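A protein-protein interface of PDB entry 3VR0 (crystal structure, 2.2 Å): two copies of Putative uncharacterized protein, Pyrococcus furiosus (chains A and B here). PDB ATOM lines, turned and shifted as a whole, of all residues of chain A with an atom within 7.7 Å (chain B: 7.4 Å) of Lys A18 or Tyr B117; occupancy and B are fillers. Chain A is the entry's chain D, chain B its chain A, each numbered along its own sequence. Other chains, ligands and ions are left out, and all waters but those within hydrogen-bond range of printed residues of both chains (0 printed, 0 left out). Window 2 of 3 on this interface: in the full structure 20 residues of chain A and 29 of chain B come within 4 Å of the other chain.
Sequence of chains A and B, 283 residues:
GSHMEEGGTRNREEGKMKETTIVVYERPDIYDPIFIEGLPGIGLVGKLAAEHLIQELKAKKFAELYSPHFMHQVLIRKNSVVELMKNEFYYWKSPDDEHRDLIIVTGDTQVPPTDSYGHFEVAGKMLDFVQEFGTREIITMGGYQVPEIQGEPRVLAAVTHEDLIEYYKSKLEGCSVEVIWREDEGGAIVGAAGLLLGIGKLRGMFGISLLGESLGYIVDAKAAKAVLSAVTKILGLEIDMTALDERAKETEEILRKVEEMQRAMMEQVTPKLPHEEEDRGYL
5 positions are printed for both chains.
Of the 14 pairs that touch across the chains among the printed residues, none has its exchanged pair printed and touching as well.
The backbone carbonyl oxygen of Val B111 is in hydrogen-bond range of a ring nitrogen (NE2) of His B119 (2.9 Å).
The side-chain hydroxyl of Thr A20 lies within hydrogen-bond range of the side-chain hydroxyl of Ser A67 (2.6 Å).
The backbone NH (N) of His A69 lies close to the side-chain hydroxyl (OG) of Ser A67 (3.1 Å).
The side-chain sulfur (SD) of Met A71 sits at hydrogen-bond distance from a ring nitrogen (ND1) of His A72 (3.7 Å).
Lys A18 touches just these residues of chain B: Glu B19 and Tyr B117.
Of the printed residues of chain A, Tyr B117 touches Lys A18 (2.8 Å) and Pro A68 (3.3 Å).
Of the printed residues of chain B, Pro A68 touches Ser B116, Tyr B117 and Phe B120.
Printed residues of chain B within 4 Å of Phe A70: Ser B116 and Phe B120.
Of the printed residues of chain B, His A72 touches Ser B116, His B119, Phe B120 and Leu B195.
Of the printed residues of chain B, Met A71 touches Ser B116.
Printed residues of chain A within 4 Å of Phe B120: Met A17, Ser A67, Pro A68, Phe A70 and His A72.
Lys B125 touches none of the printed residues of chain A.
Printed residues of chain A that touch a printed residue of chain B: Met A17, Lys A18, Ser A67, Pro A68, Phe A70, Met A71 and His A72.
Hydrophobic or aromatic side chains of chain A within 4 Å of the printed part of chain B: Met A17, Pro A68 and His A72.
Of the 16 printed residues of chain B, 6 touch a printed residue of chain A.
Hydrophobic or aromatic side chains of chain B within 4 Å of the printed part of chain A: Tyr B117, His B119, Phe B120 and Leu B195.
OE1 of Glu B19 lies within salt-bridge range of NZ of Lys A18 (3.97 Å).
ND1 of His A72 lies within hydrogen-bond range of OG of Ser B116 (2.7 Å).
The side-chain hydroxyl of Tyr B117 sits at hydrogen-bond distance from the backbone carbonyl oxygen of Lys A18 (2.8 Å).
N of Tyr B117 lies close to O of Pro A68, at 3.3 Å.
A ring nitrogen (NE2) of His A72 sits at hydrogen-bond distance from a ring nitrogen (NE2) of His B119 (3.5 Å).
Among the printed residues, pairs that only touch across the chains: Pro A68 with Phe B120 (3.4 Å), Phe A70 with Ser B116 (3.4 Å), Phe A70 with Phe B120 (3.5 Å), Met A17 with Phe B120 (3.6 Å), Pro A68 with Ser B116 (3.7 Å), Ser A67 with Phe B120 (3.8 Å), His A72 with Leu B195 (3.9 Å), His A72 with Phe B120 (3.9 Å) and Met A71 with Ser B116 (3.9 Å).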
ATOM      1  N   GLY A  15     -12.504 -22.965   0.057  1.00  0.00           N
ATOM      2  CA  GLY A  15     -12.849 -23.797  -1.145  1.00  0.00           C
ATOM      3  C   GLY A  15     -12.353 -23.115  -2.421  1.00  0.00           C
ATOM      4  O   GLY A  15     -13.155 -22.709  -3.275  1.00  0.00           O
ATOM      5  N   LYS A  16     -11.027 -22.945  -2.513  1.00  0.00           N
ATOM      6  CA  LYS A  16     -10.374 -22.442  -3.717  1.00  0.00           C
ATOM      7  C   LYS A  16     -10.461 -23.539  -4.759  1.00  0.00           C
ATOM      8  O   LYS A  16     -10.321 -24.753  -4.460  1.00  0.00           O
ATOM      9  CB  LYS A  16      -8.895 -22.089  -3.483  1.00  0.00           C
ATOM     10  CG  LYS A  16      -8.638 -20.758  -2.768  1.00  0.00           C
ATOM     11  CD  LYS A  16      -7.264 -20.798  -2.056  1.00  0.00           C
ATOM     12  CE  LYS A  16      -7.168 -19.785  -0.890  1.00  0.00           C
ATOM     13  NZ  LYS A  16      -6.308 -20.264   0.256  1.00  0.00           N
ATOM     14  N   MET A  17     -10.699 -23.113  -5.986  1.00  0.00           N
ATOM     15  CA  MET A  17     -10.826 -24.058  -7.085  1.00  0.00           C
ATOM     16  C   MET A  17      -9.773 -23.650  -8.101  1.00  0.00           C
ATOM     17  O   MET A  17     -10.108 -23.402  -9.253  1.00  0.00           O
ATOM     18  CB  MET A  17     -12.254 -24.008  -7.686  1.00  0.00           C
ATOM     19  CG  MET A  17     -13.382 -24.517  -6.755  1.00  0.00           C
ATOM     20  SD  MET A  17     -13.468 -26.331  -6.719  1.00  0.00           S
ATOM     21  CE  MET A  17     -13.870 -26.647  -8.437  1.00  0.00           C
ATOM     22  N   LYS A  18      -8.516 -23.545  -7.645  1.00  0.00           N
ATOM     23  CA  LYS A  18      -7.350 -23.322  -8.537  1.00  0.00           C
ATOM     24  C   LYS A  18      -6.965 -24.619  -9.201  1.00  0.00           C
ATOM     25  O   LYS A  18      -6.435 -24.623 -10.307  1.00  0.00           O
ATOM     26  CB  LYS A  18      -6.123 -22.767  -7.789  1.00  0.00           C
ATOM     27  CG  LYS A  18      -6.298 -21.337  -7.286  1.00  0.00           C
ATOM     28  CD  LYS A  18      -5.020 -20.530  -7.508  1.00  0.00           C
ATOM     29  CE  LYS A  18      -5.134 -19.139  -6.910  1.00  0.00           C
ATOM     30  NZ  LYS A  18      -3.772 -18.525  -6.744  1.00  0.00           N
ATOM     31  N   GLU A  19      -7.229 -25.719  -8.514  1.00  0.00           N
ATOM     32  CA  GLU A  19      -7.091 -27.032  -9.116  1.00  0.00           C
ATOM     33  C   GLU A  19      -8.096 -28.002  -8.536  1.00  0.00           C
ATOM     34  O   GLU A  19      -8.850 -27.662  -7.616  1.00  0.00           O
ATOM     35  CB  GLU A  19      -5.674 -27.572  -8.934  1.00  0.00           C
ATOM     36  CG  GLU A  19      -5.212 -27.762  -7.514  1.00  0.00           C
ATOM     37  CD  GLU A  19      -3.696 -28.008  -7.469  1.00  0.00           C
ATOM     38  OE1 GLU A  19      -2.922 -27.063  -7.777  1.00  0.00           O
ATOM     39  OE2 GLU A  19      -3.273 -29.145  -7.160  1.00  0.00           O
ATOM     40  N   THR A  20      -8.074 -29.214  -9.076  1.00  0.00           N
ATOM     41  CA  THR A  20      -8.872 -30.306  -8.576  1.00  0.00           C
ATOM     42  C   THR A  20      -8.550 -30.514  -7.078  1.00  0.00           C
ATOM     43  O   THR A  20      -7.384 -30.545  -6.678  1.00  0.00           O
ATOM     44  CB  THR A  20      -8.621 -31.562  -9.476  1.00  0.00           C
ATOM     45  OG1 THR A  20      -9.062 -31.249 -10.800  1.00  0.00           O
ATOM     46  CG2 THR A  20      -9.334 -32.826  -8.989  1.00  0.00           C
ATOM     47  N   THR A  21      -9.594 -30.584  -6.259  1.00  0.00           N
ATOM     48  CA  THR A  21      -9.417 -30.686  -4.808  1.00  0.00           C
ATOM     49  C   THR A  21     -10.354 -31.765  -4.235  1.00  0.00           C
ATOM     50  O   THR A  21     -11.527 -31.923  -4.658  1.00  0.00           O
ATOM     51  CB  THR A  21      -9.716 -29.306  -4.034  1.00  0.00           C
ATOM     52  OG1 THR A  21     -11.126 -29.144  -3.863  1.00  0.00           O
ATOM     53  CG2 THR A  21      -9.188 -28.021  -4.793  1.00  0.00           C
ATOM     54  N   SER A  67     -13.688 -30.249  -9.294  1.00  0.00           N
ATOM     55  CA  SER A  67     -12.641 -29.894 -10.257  1.00  0.00           C
ATOM     56  C   SER A  67     -13.075 -28.715 -11.106  1.00  0.00           C
ATOM     57  O   SER A  67     -14.164 -28.714 -11.616  1.00  0.00           O
ATOM     58  CB  SER A  67     -12.270 -31.085 -11.139  1.00  0.00           C
ATOM     59  OG  SER A  67     -11.294 -30.747 -12.124  1.00  0.00           O
ATOM     60  N   PRO A  68     -12.189 -27.715 -11.250  1.00  0.00           N
ATOM     61  CA  PRO A  68     -12.429 -26.577 -12.175  1.00  0.00           C
ATOM     62  C   PRO A  68     -12.296 -27.004 -13.649  1.00  0.00           C
ATOM     63  O   PRO A  68     -12.573 -26.212 -14.566  1.00  0.00           O
ATOM     64  CB  PRO A  68     -11.347 -25.578 -11.782  1.00  0.00           C
ATOM     65  CG  PRO A  68     -10.123 -26.555 -11.319  1.00  0.00           C
ATOM     66  CD  PRO A  68     -10.897 -27.627 -10.529  1.00  0.00           C
ATOM     67  N   HIS A  69     -11.898 -28.253 -13.882  1.00  0.00           N
ATOM     68  CA  HIS A  69     -11.975 -28.819 -15.225  1.00  0.00           C
ATOM     69  C   HIS A  69     -13.299 -29.508 -15.535  1.00  0.00           C
ATOM     70  O   HIS A  69     -13.492 -29.971 -16.666  1.00  0.00           O
ATOM     71  CB  HIS A  69     -10.821 -29.817 -15.465  1.00  0.00           C
ATOM     72  CG  HIS A  69      -9.487 -29.172 -15.383  1.00  0.00           C
ATOM     73  ND1 HIS A  69      -8.907 -28.558 -16.470  1.00  0.00           N
ATOM     74  CD2 HIS A  69      -8.641 -28.986 -14.343  1.00  0.00           C
ATOM     75  CE1 HIS A  69      -7.746 -28.036 -16.109  1.00  0.00           C
ATOM     76  NE2 HIS A  69      -7.565 -28.268 -14.822  1.00  0.00           N
ATOM     77  N   PHE A  70     -14.212 -29.599 -14.570  1.00  0.00           N
ATOM     78  CA  PHE A  70     -15.577 -30.090 -14.900  1.00  0.00           C
ATOM     79  C   PHE A  70     -16.350 -28.998 -15.591  1.00  0.00           C
ATOM     80  O   PHE A  70     -15.959 -27.830 -15.545  1.00  0.00           O
ATOM     81  CB  PHE A  70     -16.377 -30.615 -13.673  1.00  0.00           C
ATOM     82  CG  PHE A  70     -15.782 -31.853 -13.045  1.00  0.00           C
ATOM     83  CD1 PHE A  70     -14.969 -32.722 -13.807  1.00  0.00           C
ATOM     84  CD2 PHE A  70     -16.037 -32.164 -11.688  1.00  0.00           C
ATOM     85  CE1 PHE A  70     -14.430 -33.891 -13.234  1.00  0.00           C
ATOM     86  CE2 PHE A  70     -15.485 -33.323 -11.090  1.00  0.00           C
ATOM     87  CZ  PHE A  70     -14.669 -34.200 -11.874  1.00  0.00           C
ATOM     88  N   MET A  71     -17.447 -29.380 -16.229  1.00  0.00           N
ATOM     89  CA  MET A  71     -18.312 -28.412 -16.879  1.00  0.00           C
ATOM     90  C   MET A  71     -18.684 -27.333 -15.873  1.00  0.00           C
ATOM     91  O   MET A  71     -18.923 -27.641 -14.664  1.00  0.00           O
ATOM     92  CB  MET A  71     -19.553 -29.126 -17.448  1.00  0.00           C
ATOM     93  CG  MET A  71     -20.590 -28.184 -18.034  1.00  0.00           C
ATOM     94  SD  MET A  71     -19.902 -27.145 -19.423  1.00  0.00           S
ATOM     95  CE  MET A  71     -21.364 -26.139 -19.597  1.00  0.00           C
ATOM     96  N   HIS A  72     -18.767 -26.087 -16.380  1.00  0.00           N
ATOM     97  CA  HIS A  72     -18.943 -24.914 -15.537  1.00  0.00           C
ATOM     98  C   HIS A  72     -20.403 -24.674 -15.159  1.00  0.00           C
ATOM     99  O   HIS A  72     -21.011 -23.636 -15.474  1.00  0.00           O
ATOM    100  CB  HIS A  72     -18.302 -23.652 -16.147  1.00  0.00           C
ATOM    101  CG  HIS A  72     -18.719 -23.401 -17.564  1.00  0.00           C
ATOM    102  ND1 HIS A  72     -18.109 -24.027 -18.637  1.00  0.00           N
ATOM    103  CD2 HIS A  72     -19.668 -22.583 -18.086  1.00  0.00           C
ATOM    104  CE1 HIS A  72     -18.691 -23.625 -19.753  1.00  0.00           C
ATOM    105  NE2 HIS A  72     -19.646 -22.758 -19.442  1.00  0.00           N
ATOM    106  N   ASP A 115     -10.855 -31.441 -23.161  1.00  0.00           N
ATOM    107  CA  ASP A 115      -9.811 -30.985 -22.213  1.00  0.00           C
ATOM    108  C   ASP A 115      -8.980 -32.173 -21.769  1.00  0.00           C
ATOM    109  O   ASP A 115      -9.159 -32.681 -20.634  1.00  0.00           O
ATOM    110  CB  ASP A 115     -10.486 -30.329 -20.979  1.00  0.00           C
ATOM    111  CG  ASP A 115      -9.481 -29.799 -19.954  1.00  0.00           C
ATOM    112  OD1 ASP A 115      -8.254 -29.820 -20.211  1.00  0.00           O
ATOM    113  OD2 ASP A 115      -9.919 -29.321 -18.887  1.00  0.00           O
ATOM    114  N   GLU A 121      -5.114 -34.496 -14.953  1.00  0.00           N
ATOM    115  CA  GLU A 121      -5.099 -33.826 -13.664  1.00  0.00           C
ATOM    116  C   GLU A 121      -6.084 -34.478 -12.655  1.00  0.00           C
ATOM    117  O   GLU A 121      -5.748 -34.703 -11.468  1.00  0.00           O
ATOM    118  CB  GLU A 121      -5.389 -32.324 -13.871  1.00  0.00           C
ATOM    119  CG  GLU A 121      -4.999 -31.384 -12.741  1.00  0.00           C
ATOM    120  CD  GLU A 121      -6.188 -30.960 -11.927  1.00  0.00           C
ATOM    121  OE1 GLU A 121      -7.291 -31.450 -12.212  1.00  0.00           O
ATOM    122  OE2 GLU A 121      -6.065 -30.160 -10.991  1.00  0.00           O
ATOM    123  N   LYS A 125      -5.029 -36.697  -9.286  1.00  0.00           N
ATOM    124  CA  LYS A 125      -5.406 -36.393  -7.900  1.00  0.00           C
ATOM    125  C   LYS A 125      -6.094 -37.572  -7.241  1.00  0.00           C
ATOM    126  O   LYS A 125      -6.005 -37.725  -6.030  1.00  0.00           O
ATOM    127  CB  LYS A 125      -6.344 -35.183  -7.774  1.00  0.00           C
ATOM    128  CG  LYS A 125      -5.715 -33.828  -8.147  1.00  0.00           C
ATOM    129  CD  LYS A 125      -4.921 -33.191  -6.983  1.00  0.00           C
ATOM    130  CE  LYS A 125      -3.998 -32.056  -7.461  1.00  0.00           C
ATOM    131  NZ  LYS A 125      -4.454 -31.277  -8.701  1.00  0.00           N
ATOM    132  N   GLU B  19      -3.585 -13.303 -14.604  1.00  0.00           N
ATOM    133  CA  GLU B  19      -4.656 -13.986 -13.953  1.00  0.00           C
ATOM    134  C   GLU B  19      -5.819 -12.993 -13.903  1.00  0.00           C
ATOM    135  O   GLU B  19      -5.613 -11.793 -14.072  1.00  0.00           O
ATOM    136  CB  GLU B  19      -4.198 -14.293 -12.525  1.00  0.00           C
ATOM    137  CG  GLU B  19      -4.397 -15.708 -12.067  1.00  0.00           C
ATOM    138  CD  GLU B  19      -3.700 -15.962 -10.736  1.00  0.00           C
ATOM    139  OE1 GLU B  19      -4.401 -15.949  -9.692  1.00  0.00           O
ATOM    140  OE2 GLU B  19      -2.450 -16.153 -10.746  1.00  0.00           O
ATOM    141  N   HIS B  69      -9.294 -14.540 -19.410  1.00  0.00           N
ATOM    142  CA  HIS B  69     -10.141 -15.606 -19.911  1.00  0.00           C
ATOM    143  C   HIS B  69     -11.365 -15.048 -20.639  1.00  0.00           C
ATOM    144  O   HIS B  69     -12.163 -15.812 -21.234  1.00  0.00           O
ATOM    145  CB  HIS B  69     -10.592 -16.536 -18.772  1.00  0.00           C
ATOM    146  CG  HIS B  69      -9.478 -17.371 -18.218  1.00  0.00           C
ATOM    147  ND1 HIS B  69      -9.133 -18.585 -18.762  1.00  0.00           N
ATOM    148  CD2 HIS B  69      -8.576 -17.129 -17.238  1.00  0.00           C
ATOM    149  CE1 HIS B  69      -8.103 -19.088 -18.105  1.00  0.00           C
ATOM    150  NE2 HIS B  69      -7.747 -18.228 -17.171  1.00  0.00           N
ATOM    151  N   VAL B 111     -16.913 -15.560 -19.206  1.00  0.00           N
ATOM    152  CA  VAL B 111     -15.989 -16.401 -19.917  1.00  0.00           C
ATOM    153  C   VAL B 111     -16.716 -17.182 -21.055  1.00  0.00           C
ATOM    154  O   VAL B 111     -17.879 -17.580 -20.885  1.00  0.00           O
ATOM    155  CB  VAL B 111     -15.292 -17.326 -18.914  1.00  0.00           C
ATOM    156  CG1 VAL B 111     -14.495 -18.396 -19.600  1.00  0.00           C
ATOM    157  CG2 VAL B 111     -14.390 -16.506 -18.038  1.00  0.00           C
ATOM    158  N   THR B 114     -16.255 -22.313 -24.063  1.00  0.00           N
ATOM    159  CA  THR B 114     -15.212 -23.329 -24.315  1.00  0.00           C
ATOM    160  C   THR B 114     -14.147 -23.370 -23.243  1.00  0.00           C
ATOM    161  O   THR B 114     -13.262 -24.202 -23.292  1.00  0.00           O
ATOM    162  CB  THR B 114     -14.516 -23.080 -25.698  1.00  0.00           C
ATOM    163  OG1 THR B 114     -14.144 -21.688 -25.800  1.00  0.00           O
ATOM    164  CG2 THR B 114     -15.513 -23.407 -26.848  1.00  0.00           C
ATOM    165  N   ASP B 115     -14.228 -22.511 -22.234  1.00  0.00           N
ATOM    166  CA  ASP B 115     -13.149 -22.473 -21.248  1.00  0.00           C
ATOM    167  C   ASP B 115     -13.757 -22.607 -19.834  1.00  0.00           C
ATOM    168  O   ASP B 115     -14.043 -21.585 -19.161  1.00  0.00           O
ATOM    169  CB  ASP B 115     -12.419 -21.128 -21.403  1.00  0.00           C
ATOM    170  CG  ASP B 115     -11.340 -20.934 -20.395  1.00  0.00           C
ATOM    171  OD1 ASP B 115     -10.971 -21.931 -19.702  1.00  0.00           O
ATOM    172  OD2 ASP B 115     -10.793 -19.792 -20.329  1.00  0.00           O
ATOM    173  N   SER B 116     -13.960 -23.849 -19.384  1.00  0.00           N
ATOM    174  CA  SER B 116     -14.590 -24.067 -18.080  1.00  0.00           C
ATOM    175  C   SER B 116     -13.725 -23.587 -16.913  1.00  0.00           C
ATOM    176  O   SER B 116     -14.206 -22.921 -15.970  1.00  0.00           O
ATOM    177  CB  SER B 116     -14.996 -25.534 -17.902  1.00  0.00           C
ATOM    178  OG  SER B 116     -16.080 -25.781 -18.765  1.00  0.00           O
ATOM    179  N   TYR B 117     -12.449 -23.913 -16.990  1.00  0.00           N
ATOM    180  CA  TYR B 117     -11.524 -23.483 -16.004  1.00  0.00           C
ATOM    181  C   TYR B 117     -11.634 -21.941 -15.739  1.00  0.00           C
ATOM    182  O   TYR B 117     -11.571 -21.477 -14.618  1.00  0.00           O
ATOM    183  CB  TYR B 117     -10.104 -23.835 -16.468  1.00  0.00           C
ATOM    184  CG  TYR B 117      -9.122 -23.527 -15.360  1.00  0.00           C
ATOM    185  CD1 TYR B 117      -8.832 -24.483 -14.381  1.00  0.00           C
ATOM    186  CD2 TYR B 117      -8.539 -22.264 -15.258  1.00  0.00           C
ATOM    187  CE1 TYR B 117      -7.932 -24.205 -13.324  1.00  0.00           C
ATOM    188  CE2 TYR B 117      -7.673 -21.957 -14.199  1.00  0.00           C
ATOM    189  CZ  TYR B 117      -7.372 -22.918 -13.248  1.00  0.00           C
ATOM    190  OH  TYR B 117      -6.527 -22.584 -12.214  1.00  0.00           O
ATOM    191  N   GLY B 118     -11.735 -21.159 -16.812  1.00  0.00           N
ATOM    192  CA  GLY B 118     -11.827 -19.713 -16.643  1.00  0.00           C
ATOM    193  C   GLY B 118     -13.075 -19.310 -15.851  1.00  0.00           C
ATOM    194  O   GLY B 118     -13.023 -18.346 -15.135  1.00  0.00           O
ATOM    195  N   HIS B 119     -14.179 -20.050 -15.985  1.00  0.00           N
ATOM    196  CA  HIS B 119     -15.428 -19.691 -15.286  1.00  0.00           C
ATOM    197  C   HIS B 119     -15.205 -19.885 -13.823  1.00  0.00           C
ATOM    198  O   HIS B 119     -15.622 -19.057 -13.020  1.00  0.00           O
ATOM    199  CB  HIS B 119     -16.612 -20.580 -15.731  1.00  0.00           C
ATOM    200  CG  HIS B 119     -17.191 -20.189 -17.053  1.00  0.00           C
ATOM    201  ND1 HIS B 119     -18.264 -19.334 -17.161  1.00  0.00           N
ATOM    202  CD2 HIS B 119     -16.867 -20.556 -18.322  1.00  0.00           C
ATOM    203  CE1 HIS B 119     -18.565 -19.165 -18.439  1.00  0.00           C
ATOM    204  NE2 HIS B 119     -17.735 -19.897 -19.166  1.00  0.00           N
ATOM    205  N   PHE B 120     -14.482 -20.953 -13.485  1.00  0.00           N
ATOM    206  CA  PHE B 120     -14.145 -21.216 -12.093  1.00  0.00           C
ATOM    207  C   PHE B 120     -13.213 -20.183 -11.532  1.00  0.00           C
ATOM    208  O   PHE B 120     -13.398 -19.750 -10.377  1.00  0.00           O
ATOM    209  CB  PHE B 120     -13.537 -22.606 -11.915  1.00  0.00           C
ATOM    210  CG  PHE B 120     -14.575 -23.702 -11.933  1.00  0.00           C
ATOM    211  CD1 PHE B 120     -14.944 -24.302 -13.119  1.00  0.00           C
ATOM    212  CD2 PHE B 120     -15.167 -24.133 -10.750  1.00  0.00           C
ATOM    213  CE1 PHE B 120     -15.882 -25.311 -13.136  1.00  0.00           C
ATOM    214  CE2 PHE B 120     -16.123 -25.144 -10.782  1.00  0.00           C
ATOM    215  CZ  PHE B 120     -16.492 -25.710 -11.980  1.00  0.00           C
ATOM    216  N   GLU B 121     -12.219 -19.772 -12.337  1.00  0.00           N
ATOM    217  CA  GLU B 121     -11.310 -18.773 -11.835  1.00  0.00           C
ATOM    218  C   GLU B 121     -12.008 -17.433 -11.594  1.00  0.00           C
ATOM    219  O   GLU B 121     -11.736 -16.796 -10.595  1.00  0.00           O
ATOM    220  CB  GLU B 121     -10.047 -18.600 -12.700  1.00  0.00           C
ATOM    221  CG  GLU B 121      -9.177 -17.426 -12.236  1.00  0.00           C
ATOM    222  CD  GLU B 121      -8.015 -17.186 -13.161  1.00  0.00           C
ATOM    223  OE1 GLU B 121      -7.137 -18.080 -13.270  1.00  0.00           O
ATOM    224  OE2 GLU B 121      -7.974 -16.104 -13.779  1.00  0.00           O
ATOM    225  N   VAL B 122     -12.898 -17.023 -12.496  1.00  0.00           N
ATOM    226  CA  VAL B 122     -13.517 -15.734 -12.388  1.00  0.00           C
ATOM    227  C   VAL B 122     -14.487 -15.779 -11.182  1.00  0.00           C
ATOM    228  O   VAL B 122     -14.428 -14.923 -10.290  1.00  0.00           O
ATOM    229  CB  VAL B 122     -14.233 -15.329 -13.733  1.00  0.00           C
ATOM    230  CG1 VAL B 122     -15.273 -14.188 -13.497  1.00  0.00           C
ATOM    231  CG2 VAL B 122     -13.211 -14.905 -14.811  1.00  0.00           C
ATOM    232  N   ALA B 123     -15.341 -16.806 -11.130  1.00  0.00           N
ATOM    233  CA  ALA B 123     -16.273 -16.981  -9.991  1.00  0.00           C
ATOM    234  C   ALA B 123     -15.523 -17.008  -8.628  1.00  0.00           C
ATOM    235  O   ALA B 123     -15.890 -16.268  -7.696  1.00  0.00           O
ATOM    236  CB  ALA B 123     -17.124 -18.257 -10.191  1.00  0.00           C
ATOM    237  N   LYS B 125     -12.572 -15.675  -7.868  1.00  0.00           N
ATOM    238  CA  LYS B 125     -12.066 -14.330  -7.585  1.00  0.00           C
ATOM    239  C   LYS B 125     -13.165 -13.380  -7.082  1.00  0.00           C
ATOM    240  O   LYS B 125     -12.949 -12.584  -6.167  1.00  0.00           O
ATOM    241  CB  LYS B 125     -11.443 -13.726  -8.876  1.00  0.00           C
ATOM    242  CG  LYS B 125     -10.697 -12.487  -8.593  1.00  0.00           C
ATOM    243  CD  LYS B 125      -9.368 -12.938  -7.917  1.00  0.00           C
ATOM    244  CE  LYS B 125      -8.447 -11.795  -7.676  1.00  0.00           C
ATOM    245  NZ  LYS B 125      -7.341 -12.317  -6.812  1.00  0.00           N
ATOM    246  N   ASP B 128     -13.815 -14.455  -3.438  1.00  0.00           N
ATOM    247  CA  ASP B 128     -12.723 -13.925  -2.581  1.00  0.00           C
ATOM    248  C   ASP B 128     -12.988 -12.442  -2.277  1.00  0.00           C
ATOM    249  O   ASP B 128     -12.888 -12.013  -1.159  1.00  0.00           O
ATOM    250  CB  ASP B 128     -11.361 -13.957  -3.276  1.00  0.00           C
ATOM    251  CG  ASP B 128     -10.821 -15.326  -3.492  1.00  0.00           C
ATOM    252  OD1 ASP B 128     -11.357 -16.355  -2.982  1.00  0.00           O
ATOM    253  OD2 ASP B 128      -9.781 -15.352  -4.180  1.00  0.00           O
ATOM    254  N   LEU B 195     -22.335 -21.226 -10.663  1.00  0.00           N
ATOM    255  CA  LEU B 195     -21.014 -21.368 -10.002  1.00  0.00           C
ATOM    256  C   LEU B 195     -20.836 -20.539  -8.758  1.00  0.00           C
ATOM    257  O   LEU B 195     -20.210 -20.992  -7.810  1.00  0.00           O
ATOM    258  CB  LEU B 195     -19.842 -21.051 -10.941  1.00  0.00           C
ATOM    259  CG  LEU B 195     -19.552 -22.047 -12.080  1.00  0.00           C
ATOM    260  CD1 LEU B 195     -18.174 -21.769 -12.733  1.00  0.00           C
ATOM    261  CD2 LEU B 195     -19.595 -23.486 -11.569  1.00  0.00           C
